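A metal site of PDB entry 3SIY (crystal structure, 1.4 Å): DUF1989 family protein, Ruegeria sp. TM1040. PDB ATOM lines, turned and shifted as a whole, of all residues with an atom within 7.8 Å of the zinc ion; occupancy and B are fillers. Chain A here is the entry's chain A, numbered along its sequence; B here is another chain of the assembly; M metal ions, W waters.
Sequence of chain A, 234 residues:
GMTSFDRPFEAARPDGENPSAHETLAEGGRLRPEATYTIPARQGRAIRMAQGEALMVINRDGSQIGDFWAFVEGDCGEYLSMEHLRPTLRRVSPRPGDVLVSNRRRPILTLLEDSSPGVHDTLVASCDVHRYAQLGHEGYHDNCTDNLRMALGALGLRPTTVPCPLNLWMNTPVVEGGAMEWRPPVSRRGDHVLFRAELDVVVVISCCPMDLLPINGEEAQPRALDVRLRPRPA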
ATOM      1  N   GLN A  64      10.692  15.280  14.147  1.00  0.00           N
ATOM      2  CA  GLN A  64      10.159  15.900  12.927  1.00  0.00           C
ATOM      3  C   GLN A  64       9.419  14.891  12.052  1.00  0.00           C
ATOM      4  O   GLN A  64       9.875  13.773  11.864  1.00  0.00           O
ATOM      5  CB  GLN A  64      11.314  16.496  12.125  1.00  0.00           C
ATOM      6  CG  GLN A  64      10.909  17.202  10.859  1.00  0.00           C
ATOM      7  CD  GLN A  64       9.861  18.278  11.116  1.00  0.00           C
ATOM      8  OE1 GLN A  64       9.975  19.073  12.077  1.00  0.00           O
ATOM      9  NE2 GLN A  64       8.867  18.336  10.239  1.00  0.00           N
ATOM     10  N   ILE A  65       8.296  15.327  11.494  1.00  0.00           N
ATOM     11  CA  ILE A  65       7.540  14.511  10.541  1.00  0.00           C
ATOM     12  C   ILE A  65       8.036  14.765   9.130  1.00  0.00           C
ATOM     13  O   ILE A  65       8.264  15.944   8.777  1.00  0.00           O
ATOM     14  CB  ILE A  65       6.038  14.735  10.582  1.00  0.00           C
ATOM     15  CG1 ILE A  65       5.462  14.300  11.929  1.00  0.00           C
ATOM     16  CG2 ILE A  65       5.343  13.977   9.443  1.00  0.00           C
ATOM     17  CD1 ILE A  65       4.040  14.809  12.177  1.00  0.00           C
ATOM     18  N   GLY A  66       8.226  13.702   8.349  1.00  0.00           N
ATOM     19  CA  GLY A  66       8.516  13.861   6.926  1.00  0.00           C
ATOM     20  C   GLY A  66       7.358  13.382   6.109  1.00  0.00           C
ATOM     21  O   GLY A  66       7.090  12.183   6.112  1.00  0.00           O
ATOM     22  N   ASP A  67       6.669  14.297   5.429  1.00  0.00           N
ATOM     23  CA  ASP A  67       5.628  13.881   4.487  1.00  0.00           C
ATOM     24  C   ASP A  67       6.333  13.397   3.212  1.00  0.00           C
ATOM     25  O   ASP A  67       7.115  14.121   2.612  1.00  0.00           O
ATOM     26  CB  ASP A  67       4.654  15.041   4.163  1.00  0.00           C
ATOM     27  CG  ASP A  67       3.686  15.321   5.272  1.00  0.00           C
ATOM     28  OD1 ASP A  67       4.083  15.167   6.467  1.00  0.00           O
ATOM     29  OD2 ASP A  67       2.548  15.747   4.976  1.00  0.00           O
ATOM     30  N   TRP A  69       6.377  11.168  -0.480  1.00  0.00           N
ATOM     31  CA  TRP A  69       5.724  10.727  -1.724  1.00  0.00           C
ATOM     32  C   TRP A  69       6.734  10.080  -2.676  1.00  0.00           C
ATOM     33  O   TRP A  69       7.926  10.367  -2.587  1.00  0.00           O
ATOM     34  CB  TRP A  69       5.102  11.918  -2.445  1.00  0.00           C
ATOM     35  CG  TRP A  69       4.001  12.634  -1.793  1.00  0.00           C
ATOM     36  CD1 TRP A  69       2.651  12.392  -1.971  1.00  0.00           C
ATOM     37  CD2 TRP A  69       4.085  13.781  -0.947  1.00  0.00           C
ATOM     38  NE1 TRP A  69       1.905  13.296  -1.269  1.00  0.00           N
ATOM     39  CE2 TRP A  69       2.753  14.184  -0.660  1.00  0.00           C
ATOM     40  CE3 TRP A  69       5.155  14.527  -0.409  1.00  0.00           C
ATOM     41  CZ2 TRP A  69       2.462  15.299   0.126  1.00  0.00           C
ATOM     42  CZ3 TRP A  69       4.835  15.647   0.382  1.00  0.00           C
ATOM     43  CH2 TRP A  69       3.507  15.991   0.664  1.00  0.00           C
ATOM     44  N   ALA A 125      -4.127  13.423   5.182  1.00  0.00           N
ATOM     45  CA  ALA A 125      -3.714  14.256   4.086  1.00  0.00           C
ATOM     46  C   ALA A 125      -2.586  15.195   4.460  1.00  0.00           C
ATOM     47  O   ALA A 125      -2.484  15.626   5.630  1.00  0.00           O
ATOM     48  CB  ALA A 125      -4.882  15.103   3.588  1.00  0.00           C
ATOM     49  N   SER A 126      -1.794  15.578   3.470  1.00  0.00           N
ATOM     50  CA  SER A 126      -0.798  16.612   3.714  1.00  0.00           C
ATOM     51  C   SER A 126      -1.457  17.961   4.046  1.00  0.00           C
ATOM     52  O   SER A 126      -2.459  18.371   3.479  1.00  0.00           O
ATOM     53  CB  SER A 126       0.121  16.769   2.523  1.00  0.00           C
ATOM     54  OG  SER A 126      -0.584  16.782   1.303  1.00  0.00           O
ATOM     55  N   CYS A 127      -0.813  18.685   4.956  1.00  0.00           N
ATOM     56  CA  CYS A 127      -1.309  19.982   5.379  1.00  0.00           C
ATOM     57  C   CYS A 127      -1.227  20.933   4.175  1.00  0.00           C
ATOM     58  O   CYS A 127      -0.457  20.755   3.250  1.00  0.00           O
ATOM     59  CB  CYS A 127      -0.515  20.519   6.589  1.00  0.00           C
ATOM     60  SG  CYS A 127       1.254  20.937   6.389  1.00  0.00           S
ATOM     61  N   ASP A 128      -2.095  21.941   4.226  1.00  0.00           N
ATOM     62  CA  ASP A 128      -2.321  22.865   3.120  1.00  0.00           C
ATOM     63  C   ASP A 128      -2.856  24.178   3.690  1.00  0.00           C
ATOM     64  O   ASP A 128      -3.079  24.275   4.894  1.00  0.00           O
ATOM     65  CB  ASP A 128      -3.264  22.221   2.084  1.00  0.00           C
ATOM     66  CG  ASP A 128      -4.571  21.777   2.685  1.00  0.00           C
ATOM     67  OD1 ASP A 128      -5.182  22.571   3.456  1.00  0.00           O
ATOM     68  OD2 ASP A 128      -5.014  20.651   2.403  1.00  0.00           O
ATOM     69  N   ARG A 131      -6.060  23.877   5.842  1.00  0.00           N
ATOM     70  CA  ARG A 131      -5.820  23.363   7.165  1.00  0.00           C
ATOM     71  C   ARG A 131      -5.379  24.483   8.112  1.00  0.00           C
ATOM     72  O   ARG A 131      -5.901  24.563   9.212  1.00  0.00           O
ATOM     73  CB  ARG A 131      -4.752  22.251   7.113  1.00  0.00           C
ATOM     74  CG  ARG A 131      -4.368  21.678   8.430  1.00  0.00           C
ATOM     75  CD  ARG A 131      -5.512  20.996   9.051  1.00  0.00           C
ATOM     76  NE  ARG A 131      -5.105  20.034  10.058  1.00  0.00           N
ATOM     77  CZ  ARG A 131      -5.869  19.672  11.075  1.00  0.00           C
ATOM     78  NH1 ARG A 131      -7.076  20.203  11.216  1.00  0.00           N
ATOM     79  NH2 ARG A 131      -5.433  18.760  11.939  1.00  0.00           N
ATOM     80  N   TYR A 132      -4.433  25.331   7.691  1.00  0.00           N
ATOM     81  CA  TYR A 132      -3.946  26.394   8.571  1.00  0.00           C
ATOM     82  C   TYR A 132      -5.017  27.466   8.833  1.00  0.00           C
ATOM     83  O   TYR A 132      -5.203  27.889   9.973  1.00  0.00           O
ATOM     84  CB  TYR A 132      -2.589  26.975   8.075  1.00  0.00           C
ATOM     85  CG  TYR A 132      -1.494  25.952   8.243  1.00  0.00           C
ATOM     86  CD1 TYR A 132      -0.994  25.678   9.510  1.00  0.00           C
ATOM     87  CD2 TYR A 132      -1.026  25.215   7.161  1.00  0.00           C
ATOM     88  CE1 TYR A 132      -0.046  24.689   9.712  1.00  0.00           C
ATOM     89  CE2 TYR A 132      -0.091  24.253   7.343  1.00  0.00           C
ATOM     90  CZ  TYR A 132       0.399  23.972   8.617  1.00  0.00           C
ATOM     91  OH  TYR A 132       1.353  22.998   8.802  1.00  0.00           O
ATOM     92  N   ASP A 142       3.475  28.065   5.502  1.00  0.00           N
ATOM     93  CA  ASP A 142       4.177  27.007   4.765  1.00  0.00           C
ATOM     94  C   ASP A 142       3.367  25.733   4.968  1.00  0.00           C
ATOM     95  O   ASP A 142       2.756  25.515   6.021  1.00  0.00           O
ATOM     96  CB  ASP A 142       5.599  26.766   5.291  1.00  0.00           C
ATOM     97  CG  ASP A 142       6.542  27.936   5.055  1.00  0.00           C
ATOM     98  OD1 ASP A 142       6.606  28.415   3.904  1.00  0.00           O
ATOM     99  OD2 ASP A 142       7.260  28.287   6.016  1.00  0.00           O
ATOM    100  N   ASN A 143       3.385  24.869   3.976  1.00  0.00           N
ATOM    101  CA  ASN A 143       2.577  23.663   4.042  1.00  0.00           C
ATOM    102  C   ASN A 143       3.085  22.595   3.121  1.00  0.00           C
ATOM    103  O   ASN A 143       3.708  22.871   2.106  1.00  0.00           O
ATOM    104  CB  ASN A 143       1.094  24.008   3.790  1.00  0.00           C
ATOM    105  CG  ASN A 143       0.835  24.555   2.405  1.00  0.00           C
ATOM    106  OD1 ASN A 143       0.565  23.798   1.456  1.00  0.00           O
ATOM    107  ND2 ASN A 143       0.958  25.890   2.261  1.00  0.00           N
ATOM    108  N   CYS A 144       2.791  21.359   3.495  1.00  0.00           N
ATOM    109  CA  CYS A 144       3.354  20.194   2.811  1.00  0.00           C
ATOM    110  C   CYS A 144       2.839  20.049   1.399  1.00  0.00           C
ATOM    111  O   CYS A 144       3.580  19.657   0.489  1.00  0.00           O
ATOM    112  CB  CYS A 144       3.086  18.935   3.609  1.00  0.00           C
ATOM    113  SG  CYS A 144       4.138  18.824   5.097  1.00  0.00           S
ATOM    114  N   THR A 145       1.562  20.393   1.180  1.00  0.00           N
ATOM    115  CA  THR A 145       1.033  20.265  -0.183  1.00  0.00           C
ATOM    116  C   THR A 145       1.731  21.230  -1.146  1.00  0.00           C
ATOM    117  O   THR A 145       2.136  20.825  -2.260  1.00  0.00           O
ATOM    118  CB  THR A 145      -0.490  20.484  -0.188  1.00  0.00           C
ATOM    119  OG1 THR A 145      -1.057  19.509   0.688  1.00  0.00           O
ATOM    120  CG2 THR A 145      -1.071  20.403  -1.618  1.00  0.00           C
ATOM    121  N   ASN A 147       4.750  22.430  -0.644  1.00  0.00           N
ATOM    122  CA  ASN A 147       6.123  21.931  -0.737  1.00  0.00           C
ATOM    123  C   ASN A 147       6.246  20.820  -1.793  1.00  0.00           C
ATOM    124  O   ASN A 147       7.187  20.818  -2.564  1.00  0.00           O
ATOM    125  CB  ASN A 147       6.645  21.481   0.629  1.00  0.00           C
ATOM    126  CG  ASN A 147       6.916  22.666   1.568  1.00  0.00           C
ATOM    127  OD1 ASN A 147       6.969  23.817   1.147  1.00  0.00           O
ATOM    128  ND2 ASN A 147       7.044  22.364   2.847  1.00  0.00           N
ATOM    129  N   PRO A 165       0.214  11.644   1.608  1.00  0.00           N
ATOM    130  CA  PRO A 165       1.581  11.320   1.951  1.00  0.00           C
ATOM    131  C   PRO A 165       1.635  10.083   2.848  1.00  0.00           C
ATOM    132  O   PRO A 165       0.651   9.709   3.511  1.00  0.00           O
ATOM    133  CB  PRO A 165       2.013  12.537   2.772  1.00  0.00           C
ATOM    134  CG  PRO A 165       0.749  13.063   3.362  1.00  0.00           C
ATOM    135  CD  PRO A 165      -0.282  12.855   2.299  1.00  0.00           C
ATOM    136  N   ASN A 167       3.287   9.695   6.166  1.00  0.00           N
ATOM    137  CA  ASN A 167       3.742  10.645   7.182  1.00  0.00           C
ATOM    138  C   ASN A 167       4.755   9.979   8.095  1.00  0.00           C
ATOM    139  O   ASN A 167       4.404   9.356   9.112  1.00  0.00           O
ATOM    140  CB  ASN A 167       2.573  11.233   7.951  1.00  0.00           C
ATOM    141  CG  ASN A 167       1.587  11.906   7.054  1.00  0.00           C
ATOM    142  OD1 ASN A 167       1.933  12.884   6.379  1.00  0.00           O
ATOM    143  ND2 ASN A 167       0.351  11.397   7.017  1.00  0.00           N
ATOM    144  N   MET A 170       4.968  10.281  12.127  1.00  0.00           N
ATOM    145  CA  MET A 170       3.737  10.888  12.660  1.00  0.00           C
ATOM    146  C   MET A 170       2.970   9.895  13.535  1.00  0.00           C
ATOM    147  O   MET A 170       2.747   8.733  13.141  1.00  0.00           O
ATOM    148  CB  MET A 170       2.848  11.348  11.506  1.00  0.00           C
ATOM    149  CG  MET A 170       1.447  11.853  11.871  1.00  0.00           C
ATOM    150  SD  MET A 170       0.867  13.088  10.424  1.00  0.00           S
ATOM    151  CE  MET A 170      -0.968  13.493  10.936  1.00  0.00           C
ATOM    152  N   SER A 206       8.668  16.507   2.321  1.00  0.00           N
ATOM    153  CA  SER A 206       8.405  17.791   2.934  1.00  0.00           C
ATOM    154  C   SER A 206       8.581  17.705   4.439  1.00  0.00           C
ATOM    155  O   SER A 206       8.021  16.809   5.088  1.00  0.00           O
ATOM    156  CB  SER A 206       6.976  18.246   2.663  1.00  0.00           C
ATOM    157  OG  SER A 206       6.663  19.451   3.340  1.00  0.00           O
ATOM    158  N   CYS A 207       9.407  18.598   4.982  1.00  0.00           N
ATOM    159  CA  CYS A 207       9.555  18.746   6.442  1.00  0.00           C
ATOM    160  C   CYS A 207       8.357  19.496   6.944  1.00  0.00           C
ATOM    161  O   CYS A 207       8.255  20.711   6.784  1.00  0.00           O
ATOM    162  CB  CYS A 207      10.874  19.473   6.763  1.00  0.00           C
ATOM    163  SG  CYS A 207      12.292  18.487   6.294  1.00  0.00           S
ATOM    164  N   CYS A 208       7.385  18.759   7.493  1.00  0.00           N
ATOM    165  CA  CYS A 208       6.115  19.368   7.844  1.00  0.00           C
ATOM    166  C   CYS A 208       6.301  20.601   8.739  1.00  0.00           C
ATOM    167  O   CYS A 208       6.970  20.517   9.772  1.00  0.00           O
ATOM    168  CB  CYS A 208       5.241  18.353   8.571  1.00  0.00           C
ATOM    169  SG  CYS A 208       3.591  18.965   8.926  1.00  0.00           S
ATOM    170  N   PRO A 209       5.689  21.730   8.373  1.00  0.00           N
ATOM    171  CA  PRO A 209       5.808  22.936   9.170  1.00  0.00           C
ATOM    172  C   PRO A 209       4.712  23.100  10.222  1.00  0.00           C
ATOM    173  O   PRO A 209       4.585  24.173  10.791  1.00  0.00           O
ATOM    174  CB  PRO A 209       5.719  24.068   8.123  1.00  0.00           C
ATOM    175  CG  PRO A 209       4.894  23.517   7.059  1.00  0.00           C
ATOM    176  CD  PRO A 209       5.139  22.015   7.026  1.00  0.00           C
ATOM    177  N   MET A 210       3.949  22.059  10.518  1.00  0.00           N
ATOM    178  CA  MET A 210       2.867  22.204  11.478  1.00  0.00           C
ATOM    179  C   MET A 210       3.441  22.630  12.817  1.00  0.00           C
ATOM    180  O   MET A 210       4.248  21.929  13.428  1.00  0.00           O
ATOM    181  CB  MET A 210       2.094  20.892  11.644  1.00  0.00           C
ATOM    182  CG  MET A 210       1.034  20.924  12.721  1.00  0.00           C
ATOM    183  SD  MET A 210      -0.367  22.206  12.494  1.00  0.00           S
ATOM    184  CE  MET A 210      -1.014  21.576  10.762  1.00  0.00           C
ATOM    185  N   ILE A 215       2.458  17.686  16.640  1.00  0.00           N
ATOM    186  CA  ILE A 215       2.810  16.517  15.862  1.00  0.00           C
ATOM    187  C   ILE A 215       4.281  16.474  15.464  1.00  0.00           C
ATOM    188  O   ILE A 215       4.809  15.401  15.172  1.00  0.00           O
ATOM    189  CB  ILE A 215       1.862  16.336  14.654  1.00  0.00           C
ATOM    190  CG1 ILE A 215       2.053  17.444  13.611  1.00  0.00           C
ATOM    191  CG2 ILE A 215       0.409  16.249  15.136  1.00  0.00           C
ATOM    192  CD1 ILE A 215       1.223  17.232  12.332  1.00  0.00           C
ATOM    193  N   ASN A 216       4.941  17.640  15.445  1.00  0.00           N
ATOM    194  CA  ASN A 216       6.400  17.745  15.264  1.00  0.00           C
ATOM    195  C   ASN A 216       7.160  17.958  16.569  1.00  0.00           C
ATOM    196  O   ASN A 216       8.274  18.516  16.606  1.00  0.00           O
ATOM    197  CB  ASN A 216       6.687  18.887  14.284  1.00  0.00           C
ATOM    198  CG  ASN A 216       6.237  18.556  12.888  1.00  0.00           C
ATOM    199  OD1 ASN A 216       6.641  17.555  12.311  1.00  0.00           O
ATOM    200  ND2 ASN A 216       5.380  19.420  12.312  1.00  0.00           N
ATOM    201  N   ARG B 105     -10.973  20.777   1.813  1.00  0.00           N
ATOM    202  CA  ARG B 105     -11.379  20.841   3.223  1.00  0.00           C
ATOM    203  C   ARG B 105     -12.636  21.670   3.413  1.00  0.00           C
ATOM    204  O   ARG B 105     -12.908  22.105   4.517  1.00  0.00           O
ATOM    205  CB  ARG B 105     -10.258  21.325   4.157  1.00  0.00           C
ATOM    206  CG  ARG B 105      -9.067  20.455   4.082  1.00  0.00           C
ATOM    207  CD  ARG B 105      -8.051  20.811   5.136  1.00  0.00           C
ATOM    208  NE  ARG B 105      -6.738  20.293   4.762  1.00  0.00           N
ATOM    209  CZ  ARG B 105      -6.092  19.282   5.341  1.00  0.00           C
ATOM    210  NH1 ARG B 105      -6.586  18.621   6.376  1.00  0.00           N
ATOM    211  NH2 ARG B 105      -4.892  18.938   4.879  1.00  0.00           N
HETATM  212 ZN    ZN M   1       2.623  19.119   6.834  1.00  0.00          ZN
HETATM  213  O   HOH W   1       1.349  17.535   6.552  1.00  0.00           O
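N of Met 210 sits close to SG of Cys 208 (3.5 Å). O of Cys 208 lies within hydrogen-bond range of ND2 of Asn 216. N of Cys 208 sits at hydrogen-bond distance from O of Ile 65 (3.2 Å). The side-chain carboxylate (OD1) of Asp 67 lies close to the side-chain amide oxygen (OD1) of Asn 167 (3.1 Å). The backbone carbonyl oxygen of Asp 67 sits at hydrogen-bond distance from the backbone NH of Ser 206, 2.9 Å away. The side-chain sulfur of Cys 144 sits close to the side-chain hydroxyl of Ser 206 (3.1 Å). SG of Cys 144 lies close to OD2 of Asp 67. OH of Tyr 132 sits close to SG of Cys 127, at 3.2 Å.
Water W1 lies within hydrogen-bond range of the side-chain carboxylate (OD2) of Asp 67 (2.7 Å) and the backbone NH (N) of Cys 127 (2.9 Å).
Merely in contact with the zinc ion: Asp 67 (3.9 Å) and Pro 209 (3.8 Å). Five residues have an atom within 4 Å of the zinc ion: Asp 67, Cys 127, Cys 144, Cys 208 and Pro 209. Along chain A the residues within 4 Å of the zinc ion span positions 67 to 209.
Water W1 binds the zinc ion, 2.1 Å away. SG of Cys 208 binds the zinc ion. The side-chain sulfur (SG) of Cys 127 binds the zinc ion. The zinc ion is bound by SG of Cys 144 (2.3 Å). The zinc ion has four donor atoms within binding distance.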
